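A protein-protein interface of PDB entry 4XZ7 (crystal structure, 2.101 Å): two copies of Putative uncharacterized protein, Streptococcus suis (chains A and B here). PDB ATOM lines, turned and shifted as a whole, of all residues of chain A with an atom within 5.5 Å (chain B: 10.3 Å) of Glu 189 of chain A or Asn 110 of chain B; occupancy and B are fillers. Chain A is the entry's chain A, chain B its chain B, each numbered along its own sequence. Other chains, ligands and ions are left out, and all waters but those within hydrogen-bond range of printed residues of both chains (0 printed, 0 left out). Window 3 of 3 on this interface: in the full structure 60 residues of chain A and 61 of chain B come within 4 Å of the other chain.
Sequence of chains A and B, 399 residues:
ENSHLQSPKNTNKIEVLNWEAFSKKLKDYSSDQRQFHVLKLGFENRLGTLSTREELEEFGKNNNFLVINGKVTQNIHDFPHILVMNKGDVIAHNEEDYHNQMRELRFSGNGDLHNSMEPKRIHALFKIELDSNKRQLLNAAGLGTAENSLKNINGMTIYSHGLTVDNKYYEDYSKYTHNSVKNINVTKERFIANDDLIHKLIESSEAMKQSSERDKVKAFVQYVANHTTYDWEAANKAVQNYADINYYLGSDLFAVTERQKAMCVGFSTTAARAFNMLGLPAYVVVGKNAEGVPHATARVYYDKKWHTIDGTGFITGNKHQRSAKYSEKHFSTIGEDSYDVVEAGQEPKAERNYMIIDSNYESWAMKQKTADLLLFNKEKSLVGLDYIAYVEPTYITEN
No position is printed for both chains.
Of the 11 pairs that touch across the chains among the printed residues, none has its exchanged pair printed and touching as well.
N of Ser 108 of chain B sits at hydrogen-bond distance from O of Val 186 of chain A.
The backbone NH of Gly 109 of chain B is in hydrogen-bond range of the backbone carbonyl oxygen of Val 186 of chain A (2.9 Å).
The side-chain carboxylate (OD1) of Asp 166 of chain B lies within hydrogen-bond range of the backbone NH (N) of Val 186 of chain A, at 2.9 Å.
The backbone NH (N) of Lys 188 of chain A is in hydrogen-bond range of the side-chain amide oxygen (OD1) of Asn 110 of chain B (2.8 Å).
OE1 of Glu 189 of chain A sits at hydrogen-bond distance from ND2 of Asn 110 of chain B, at 3.1 Å.
Val 186 of chain A touches Phe 107 of chain B (O to CB, 3.3 Å).
CB of Phe 107 of chain B touches C of Thr 187 of chain A (3.9 Å).
CG2 of Thr 187 of chain A touches CA of Gly 109 of chain B (3.8 Å).
Asn 110 of chain B touches Thr 187 of chain A (OD1 to C, 3.6 Å).
Lys 188 of chain A touches Phe 107 of chain B.
CZ of Phe 107 of chain B touches CG of Phe 191 of chain A (3.6 Å).
The side-chain hydroxyl (OG1) of Thr 187 of chain A lies within hydrogen-bond range of the backbone NH (N) of Arg 190 of chain A (2.9 Å).
N of Ser 108 of chain B is in hydrogen-bond range of O of Val 165 of chain B (3.1 Å).
NZ of Lys 188 of chain A is in salt-bridge range of OE2 of Glu 189 of chain A (2.6 Å).
The side-chain hydroxyl (OG) of Ser 108 of chain B lies within hydrogen-bond range of the backbone carbonyl oxygen (O) of Met 117 of chain B, 2.7 Å away.
The backbone NH (N) of Glu 189 of chain A lies close to the side-chain hydroxyl (OG1) of Thr 187 of chain A (3.5 Å).
Glu 189 of chain A touches just one residue of chain B: Asn 110 (3.1 Å).
Thr 187 of chain A touches just these residues of chain B: Phe 107, Gly 109 and Asn 110.
Lys 188 of chain A touches just these residues of chain B: Phe 107 (3.6 Å) and Asn 110 (2.8 Å).
No residue of chain B comes within 4 Å of Ile 192 of chain A.
No residue of chain B comes within 4 Å of Ala 193 of chain A.
Of the printed residues of chain A, Asp 166 of chain B touches Val 186.
Printed residues of chain A within 4 Å of Gly 109 of chain B: Val 186 and Thr 187.
Of the printed residues of chain B, Phe 191 of chain A touches Phe 107.
Glu 118 of chain B touches none of the printed residues of chain A.
The nearest residue of chain B that does not touch Glu 189 of chain A is Phe 107 of chain B (6.2 Å).
The nearest residue of chain A that does not touch Asn 110 of chain B is Val 186 of chain A (4.7 Å).
The nearest printed residue of chain B that does not touch Val 186 of chain A is Val 165 of chain B (4.6 Å).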
ATOM      1  N   VAL A 186      26.964   9.979  10.059  1.00  0.00           N
ATOM      2  CA  VAL A 186      27.049   9.070   8.927  1.00  0.00           C
ATOM      3  C   VAL A 186      25.725   9.053   8.165  1.00  0.00           C
ATOM      4  O   VAL A 186      24.648   8.987   8.783  1.00  0.00           O
ATOM      5  CB  VAL A 186      27.433   7.641   9.400  1.00  0.00           C
ATOM      6  CG1 VAL A 186      27.360   6.659   8.247  1.00  0.00           C
ATOM      7  CG2 VAL A 186      28.835   7.663  10.043  1.00  0.00           C
ATOM      8  N   THR A 187      25.810   9.156   6.830  1.00  0.00           N
ATOM      9  CA  THR A 187      24.642   9.034   5.960  1.00  0.00           C
ATOM     10  C   THR A 187      24.428   7.577   5.535  1.00  0.00           C
ATOM     11  O   THR A 187      25.357   6.778   5.573  1.00  0.00           O
ATOM     12  CB  THR A 187      24.795   9.866   4.683  1.00  0.00           C
ATOM     13  OG1 THR A 187      25.844   9.300   3.896  1.00  0.00           O
ATOM     14  CG2 THR A 187      25.127  11.325   5.000  1.00  0.00           C
ATOM     15  N   LYS A 188      23.230   7.227   5.081  1.00  0.00           N
ATOM     16  CA  LYS A 188      23.011   5.851   4.632  1.00  0.00           C
ATOM     17  C   LYS A 188      23.869   5.565   3.390  1.00  0.00           C
ATOM     18  O   LYS A 188      24.350   4.451   3.182  1.00  0.00           O
ATOM     19  CB  LYS A 188      21.526   5.590   4.351  1.00  0.00           C
ATOM     20  CG  LYS A 188      20.950   6.325   3.145  1.00  0.00           C
ATOM     21  CD  LYS A 188      19.478   5.959   2.969  1.00  0.00           C
ATOM     22  CE  LYS A 188      18.927   6.455   1.644  1.00  0.00           C
ATOM     23  NZ  LYS A 188      19.238   7.893   1.432  1.00  0.00           N
ATOM     24  N   GLU A 189      24.087   6.585   2.576  1.00  0.00           N
ATOM     25  CA  GLU A 189      24.951   6.429   1.411  1.00  0.00           C
ATOM     26  C   GLU A 189      26.397   6.079   1.809  1.00  0.00           C
ATOM     27  O   GLU A 189      27.028   5.192   1.221  1.00  0.00           O
ATOM     28  CB  GLU A 189      24.921   7.705   0.583  1.00  0.00           C
ATOM     29  CG  GLU A 189      23.593   7.957  -0.118  1.00  0.00           C
ATOM     30  CD  GLU A 189      22.548   8.617   0.765  1.00  0.00           C
ATOM     31  OE1 GLU A 189      22.848   8.960   1.930  1.00  0.00           O
ATOM     32  OE2 GLU A 189      21.412   8.794   0.278  1.00  0.00           O
ATOM     33  N   ARG A 190      26.926   6.789   2.801  1.00  0.00           N
ATOM     34  CA  ARG A 190      28.258   6.495   3.330  1.00  0.00           C
ATOM     35  C   ARG A 190      28.329   5.074   3.880  1.00  0.00           C
ATOM     36  O   ARG A 190      29.335   4.364   3.701  1.00  0.00           O
ATOM     37  CB  ARG A 190      28.624   7.486   4.438  1.00  0.00           C
ATOM     38  CG  ARG A 190      30.000   7.262   5.082  1.00  0.00           C
ATOM     39  CD  ARG A 190      31.119   7.949   4.276  1.00  0.00           C
ATOM     40  NE  ARG A 190      32.384   7.925   5.015  1.00  0.00           N
ATOM     41  CZ  ARG A 190      32.678   8.744   6.023  1.00  0.00           C
ATOM     42  NH1 ARG A 190      31.800   9.661   6.429  1.00  0.00           N
ATOM     43  NH2 ARG A 190      33.850   8.637   6.638  1.00  0.00           N
ATOM     44  N   PHE A 191      27.266   4.661   4.560  1.00  0.00           N
ATOM     45  CA  PHE A 191      27.280   3.344   5.190  1.00  0.00           C
ATOM     46  C   PHE A 191      27.288   2.283   4.089  1.00  0.00           C
ATOM     47  O   PHE A 191      28.067   1.325   4.131  1.00  0.00           O
ATOM     48  CB  PHE A 191      26.088   3.146   6.133  1.00  0.00           C
ATOM     49  CG  PHE A 191      26.147   1.847   6.904  1.00  0.00           C
ATOM     50  CD1 PHE A 191      26.838   1.772   8.111  1.00  0.00           C
ATOM     51  CD2 PHE A 191      25.530   0.706   6.423  1.00  0.00           C
ATOM     52  CE1 PHE A 191      26.912   0.591   8.808  1.00  0.00           C
ATOM     53  CE2 PHE A 191      25.599  -0.493   7.123  1.00  0.00           C
ATOM     54  CZ  PHE A 191      26.287  -0.555   8.306  1.00  0.00           C
ATOM     55  N   ILE A 192      26.446   2.480   3.081  1.00  0.00           N
ATOM     56  CA  ILE A 192      26.363   1.528   1.977  1.00  0.00           C
ATOM     57  C   ILE A 192      27.689   1.463   1.213  1.00  0.00           C
ATOM     58  O   ILE A 192      28.155   0.368   0.824  1.00  0.00           O
ATOM     59  CB  ILE A 192      25.204   1.889   1.038  1.00  0.00           C
ATOM     60  CG1 ILE A 192      23.873   1.694   1.775  1.00  0.00           C
ATOM     61  CG2 ILE A 192      25.253   1.058  -0.240  1.00  0.00           C
ATOM     62  CD1 ILE A 192      22.632   2.189   0.987  1.00  0.00           C
ATOM     63  N   ALA A 193      28.329   2.623   1.023  1.00  0.00           N
ATOM     64  CA  ALA A 193      29.620   2.632   0.337  1.00  0.00           C
ATOM     65  C   ALA A 193      30.669   1.906   1.202  1.00  0.00           C
ATOM     66  O   ALA A 193      31.592   1.251   0.692  1.00  0.00           O
ATOM     67  CB  ALA A 193      30.055   4.053   0.027  1.00  0.00           C
ATOM     68  N   ASN A 194      30.511   1.981   2.517  1.00  0.00           N
ATOM     69  CA  ASN A 194      31.441   1.260   3.363  1.00  0.00           C
ATOM     70  C   ASN A 194      31.249  -0.245   3.227  1.00  0.00           C
ATOM     71  O   ASN A 194      32.236  -0.996   3.155  1.00  0.00           O
ATOM     72  CB  ASN A 194      31.310   1.685   4.811  1.00  0.00           C
ATOM     73  CG  ASN A 194      32.466   1.203   5.650  1.00  0.00           C
ATOM     74  OD1 ASN A 194      33.615   1.606   5.444  1.00  0.00           O
ATOM     75  ND2 ASN A 194      32.174   0.327   6.606  1.00  0.00           N
ATOM     76  N   GLU B 104      13.152   0.919   8.940  1.00  0.00           N
ATOM     77  CA  GLU B 104      14.458   0.989   8.321  1.00  0.00           C
ATOM     78  C   GLU B 104      15.328   1.817   9.247  1.00  0.00           C
ATOM     79  O   GLU B 104      14.853   2.791   9.824  1.00  0.00           O
ATOM     80  CB  GLU B 104      14.351   1.609   6.915  1.00  0.00           C
ATOM     81  CG  GLU B 104      15.658   2.085   6.269  1.00  0.00           C
ATOM     82  CD  GLU B 104      15.485   2.456   4.785  1.00  0.00           C
ATOM     83  OE1 GLU B 104      16.183   3.382   4.297  1.00  0.00           O
ATOM     84  OE2 GLU B 104      14.655   1.810   4.102  1.00  0.00           O
ATOM     85  N   LEU B 105      16.578   1.413   9.425  1.00  0.00           N
ATOM     86  CA  LEU B 105      17.516   2.230  10.185  1.00  0.00           C
ATOM     87  C   LEU B 105      17.506   3.648   9.630  1.00  0.00           C
ATOM     88  O   LEU B 105      17.506   3.843   8.416  1.00  0.00           O
ATOM     89  CB  LEU B 105      18.932   1.665  10.113  1.00  0.00           C
ATOM     90  CG  LEU B 105      19.273   0.310  10.717  1.00  0.00           C
ATOM     91  CD1 LEU B 105      20.789   0.198  10.710  1.00  0.00           C
ATOM     92  CD2 LEU B 105      18.738   0.169  12.134  1.00  0.00           C
ATOM     93  N   ARG B 106      17.505   4.620  10.530  1.00  0.00           N
ATOM     94  CA  ARG B 106      17.537   6.042  10.188  1.00  0.00           C
ATOM     95  C   ARG B 106      18.916   6.614  10.496  1.00  0.00           C
ATOM     96  O   ARG B 106      19.314   6.662  11.656  1.00  0.00           O
ATOM     97  CB  ARG B 106      16.469   6.781  10.985  1.00  0.00           C
ATOM     98  CG  ARG B 106      16.474   8.278  10.833  1.00  0.00           C
ATOM     99  CD  ARG B 106      15.306   8.708   9.976  1.00  0.00           C
ATOM    100  NE  ARG B 106      14.054   8.075  10.389  1.00  0.00           N
ATOM    101  CZ  ARG B 106      13.046   8.717  10.977  1.00  0.00           C
ATOM    102  NH1 ARG B 106      13.136  10.020  11.235  1.00  0.00           N
ATOM    103  NH2 ARG B 106      11.943   8.054  11.303  1.00  0.00           N
ATOM    104  N   PHE B 107      19.658   7.015   9.471  1.00  0.00           N
ATOM    105  CA  PHE B 107      21.033   7.464   9.668  1.00  0.00           C
ATOM    106  C   PHE B 107      21.089   8.963   9.942  1.00  0.00           C
ATOM    107  O   PHE B 107      20.373   9.739   9.311  1.00  0.00           O
ATOM    108  CB  PHE B 107      21.902   7.107   8.446  1.00  0.00           C
ATOM    109  CG  PHE B 107      22.348   5.674   8.430  1.00  0.00           C
ATOM    110  CD1 PHE B 107      21.506   4.676   7.944  1.00  0.00           C
ATOM    111  CD2 PHE B 107      23.588   5.320   8.931  1.00  0.00           C
ATOM    112  CE1 PHE B 107      21.907   3.349   7.950  1.00  0.00           C
ATOM    113  CE2 PHE B 107      23.995   4.005   8.934  1.00  0.00           C
ATOM    114  CZ  PHE B 107      23.148   3.011   8.448  1.00  0.00           C
ATOM    115  N   SER B 108      21.957   9.348  10.876  1.00  0.00           N
ATOM    116  CA  SER B 108      22.071  10.724  11.352  1.00  0.00           C
ATOM    117  C   SER B 108      22.240  11.749  10.227  1.00  0.00           C
ATOM    118  O   SER B 108      21.572  12.776  10.210  1.00  0.00           O
ATOM    119  CB  SER B 108      23.250  10.832  12.327  1.00  0.00           C
ATOM    120  OG  SER B 108      23.296  12.103  12.945  1.00  0.00           O
ATOM    121  N   GLY B 109      23.138  11.463   9.296  1.00  0.00           N
ATOM    122  CA  GLY B 109      23.408  12.375   8.195  1.00  0.00           C
ATOM    123  C   GLY B 109      22.259  12.650   7.226  1.00  0.00           C
ATOM    124  O   GLY B 109      22.311  13.621   6.457  1.00  0.00           O
ATOM    125  N   ASN B 110      21.224  11.813   7.240  1.00  0.00           N
ATOM    126  CA  ASN B 110      20.095  12.036   6.327  1.00  0.00           C
ATOM    127  C   ASN B 110      18.955  12.867   6.947  1.00  0.00           C
ATOM    128  O   ASN B 110      17.895  13.025   6.338  1.00  0.00           O
ATOM    129  CB  ASN B 110      19.530  10.699   5.820  1.00  0.00           C
ATOM    130  CG  ASN B 110      20.541   9.894   5.016  1.00  0.00           C
ATOM    131  OD1 ASN B 110      21.047   8.881   5.494  1.00  0.00           O
ATOM    132  ND2 ASN B 110      20.827  10.328   3.788  1.00  0.00           N
ATOM    133  N   GLY B 111      19.161  13.384   8.155  1.00  0.00           N
ATOM    134  CA  GLY B 111      18.194  14.293   8.754  1.00  0.00           C
ATOM    135  C   GLY B 111      17.980  15.519   7.877  1.00  0.00           C
ATOM    136  O   GLY B 111      18.911  15.979   7.206  1.00  0.00           O
ATOM    137  N   ASP B 112      16.757  16.044   7.867  1.00  0.00           N
ATOM    138  CA  ASP B 112      16.428  17.197   7.020  1.00  0.00           C
ATOM    139  C   ASP B 112      17.202  18.436   7.460  1.00  0.00           C
ATOM    140  O   ASP B 112      17.989  18.999   6.692  1.00  0.00           O
ATOM    141  CB  ASP B 112      14.918  17.474   7.046  1.00  0.00           C
ATOM    142  N   LEU B 113      16.971  18.847   8.706  1.00  0.00           N
ATOM    143  CA  LEU B 113      17.601  20.033   9.271  1.00  0.00           C
ATOM    144  C   LEU B 113      19.099  19.811   9.459  1.00  0.00           C
ATOM    145  O   LEU B 113      19.527  19.088  10.364  1.00  0.00           O
ATOM    146  CB  LEU B 113      16.939  20.404  10.593  1.00  0.00           C
ATOM    147  N   HIS B 114      19.887  20.441   8.590  1.00  0.00           N
ATOM    148  CA  HIS B 114      21.334  20.256   8.557  1.00  0.00           C
ATOM    149  C   HIS B 114      22.025  20.651   9.865  1.00  0.00           C
ATOM    150  O   HIS B 114      23.047  20.068  10.232  1.00  0.00           O
ATOM    151  CB  HIS B 114      21.928  21.045   7.390  1.00  0.00           C
ATOM    152  N   ASN B 115      21.461  21.626  10.574  1.00  0.00           N
ATOM    153  CA  ASN B 115      22.139  22.234  11.724  1.00  0.00           C
ATOM    154  C   ASN B 115      22.228  21.335  12.964  1.00  0.00           C
ATOM    155  O   ASN B 115      23.147  21.489  13.775  1.00  0.00           O
ATOM    156  CB  ASN B 115      21.455  23.551  12.090  1.00  0.00           C
ATOM    157  N   SER B 116      21.285  20.410  13.121  1.00  0.00           N
ATOM    158  CA  SER B 116      21.263  19.567  14.316  1.00  0.00           C
ATOM    159  C   SER B 116      21.225  18.086  13.961  1.00  0.00           C
ATOM    160  O   SER B 116      20.169  17.535  13.624  1.00  0.00           O
ATOM    161  CB  SER B 116      20.078  19.931  15.207  1.00  0.00           C
ATOM    162  N   MET B 117      22.387  17.445  14.044  1.00  0.00           N
ATOM    163  CA  MET B 117      22.494  16.030  13.722  1.00  0.00           C
ATOM    164  C   MET B 117      23.108  15.231  14.876  1.00  0.00           C
ATOM    165  O   MET B 117      23.684  14.158  14.666  1.00  0.00           O
ATOM    166  CB  MET B 117      23.300  15.836  12.434  1.00  0.00           C
ATOM    167  CG  MET B 117      22.560  16.320  11.198  1.00  0.00           C
ATOM    168  SD  MET B 117      23.501  16.111   9.675  1.00  0.00           S
ATOM    169  CE  MET B 117      22.267  16.590   8.457  1.00  0.00           C
ATOM    170  N   GLU B 118      22.987  15.769  16.090  1.00  0.00           N
ATOM    171  CA  GLU B 118      23.203  14.985  17.306  1.00  0.00           C
ATOM    172  C   GLU B 118      22.124  13.908  17.342  1.00  0.00           C
ATOM    173  O   GLU B 118      21.057  14.103  16.769  1.00  0.00           O
ATOM    174  CB  GLU B 118      23.134  15.859  18.559  1.00  0.00           C
ATOM    175  CG  GLU B 118      21.721  16.333  18.931  1.00  0.00           C
ATOM    176  CD  GLU B 118      21.174  17.406  17.993  1.00  0.00           C
ATOM    177  OE1 GLU B 118      21.957  17.952  17.181  1.00  0.00           O
ATOM    178  OE2 GLU B 118      19.959  17.702  18.067  1.00  0.00           O
ATOM    179  N   LYS B 120      19.026  11.795  17.440  1.00  0.00           N
ATOM    180  CA  LYS B 120      17.608  12.015  17.700  1.00  0.00           C
ATOM    181  C   LYS B 120      16.993  10.838  18.462  1.00  0.00           C
ATOM    182  O   LYS B 120      17.483   9.699  18.393  1.00  0.00           O
ATOM    183  CB  LYS B 120      16.853  12.241  16.388  1.00  0.00           C
ATOM    184  CG  LYS B 120      17.402  13.401  15.568  1.00  0.00           C
ATOM    185  CD  LYS B 120      17.672  14.615  16.462  1.00  0.00           C
ATOM    186  CE  LYS B 120      18.545  15.667  15.778  1.00  0.00           C
ATOM    187  NZ  LYS B 120      17.876  16.282  14.599  1.00  0.00           N
ATOM    188  N   LEU B 163      16.512   7.122  17.835  1.00  0.00           N
ATOM    189  CA  LEU B 163      15.867   7.036  16.539  1.00  0.00           C
ATOM    190  C   LEU B 163      16.928   6.970  15.443  1.00  0.00           C
ATOM    191  O   LEU B 163      16.860   6.112  14.578  1.00  0.00           O
ATOM    192  CB  LEU B 163      14.930   8.226  16.295  1.00  0.00           C
ATOM    193  CG  LEU B 163      14.223   8.245  14.934  1.00  0.00           C
ATOM    194  CD1 LEU B 163      13.510   6.918  14.662  1.00  0.00           C
ATOM    195  CD2 LEU B 163      13.232   9.385  14.866  1.00  0.00           C
ATOM    196  N   THR B 164      17.908   7.873  15.485  1.00  0.00           N
ATOM    197  CA  THR B 164      18.980   7.849  14.490  1.00  0.00           C
ATOM    198  C   THR B 164      20.132   6.955  14.940  1.00  0.00           C
ATOM    199  O   THR B 164      20.414   6.826  16.137  1.00  0.00           O
ATOM    200  CB  THR B 164      19.554   9.249  14.211  1.00  0.00           C
ATOM    201  OG1 THR B 164      20.023   9.790  15.441  1.00  0.00           O
ATOM    202  CG2 THR B 164      18.481  10.187  13.616  1.00  0.00           C
ATOM    203  N   VAL B 165      20.789   6.343  13.965  1.00  0.00           N
ATOM    204  CA  VAL B 165      21.997   5.585  14.217  1.00  0.00           C
ATOM    205  C   VAL B 165      23.178   6.373  13.654  1.00  0.00           C
ATOM    206  O   VAL B 165      23.025   7.155  12.710  1.00  0.00           O
ATOM    207  CB  VAL B 165      21.923   4.162  13.595  1.00  0.00           C
ATOM    208  CG1 VAL B 165      20.727   3.419  14.152  1.00  0.00           C
ATOM    209  CG2 VAL B 165      21.828   4.230  12.095  1.00  0.00           C
ATOM    210  N   ASP B 166      24.340   6.195  14.266  1.00  0.00           N
ATOM    211  CA  ASP B 166      25.536   6.897  13.836  1.00  0.00           C
ATOM    212  C   ASP B 166      26.724   6.064  14.272  1.00  0.00           C
ATOM    213  O   ASP B 166      26.571   5.074  15.003  1.00  0.00           O
ATOM    214  CB  ASP B 166      25.607   8.299  14.457  1.00  0.00           C
ATOM    215  CG  ASP B 166      26.461   9.272  13.645  1.00  0.00           C
ATOM    216  OD1 ASP B 166      27.197   8.835  12.733  1.00  0.00           O
ATOM    217  OD2 ASP B 166      26.394  10.485  13.937  1.00  0.00           O
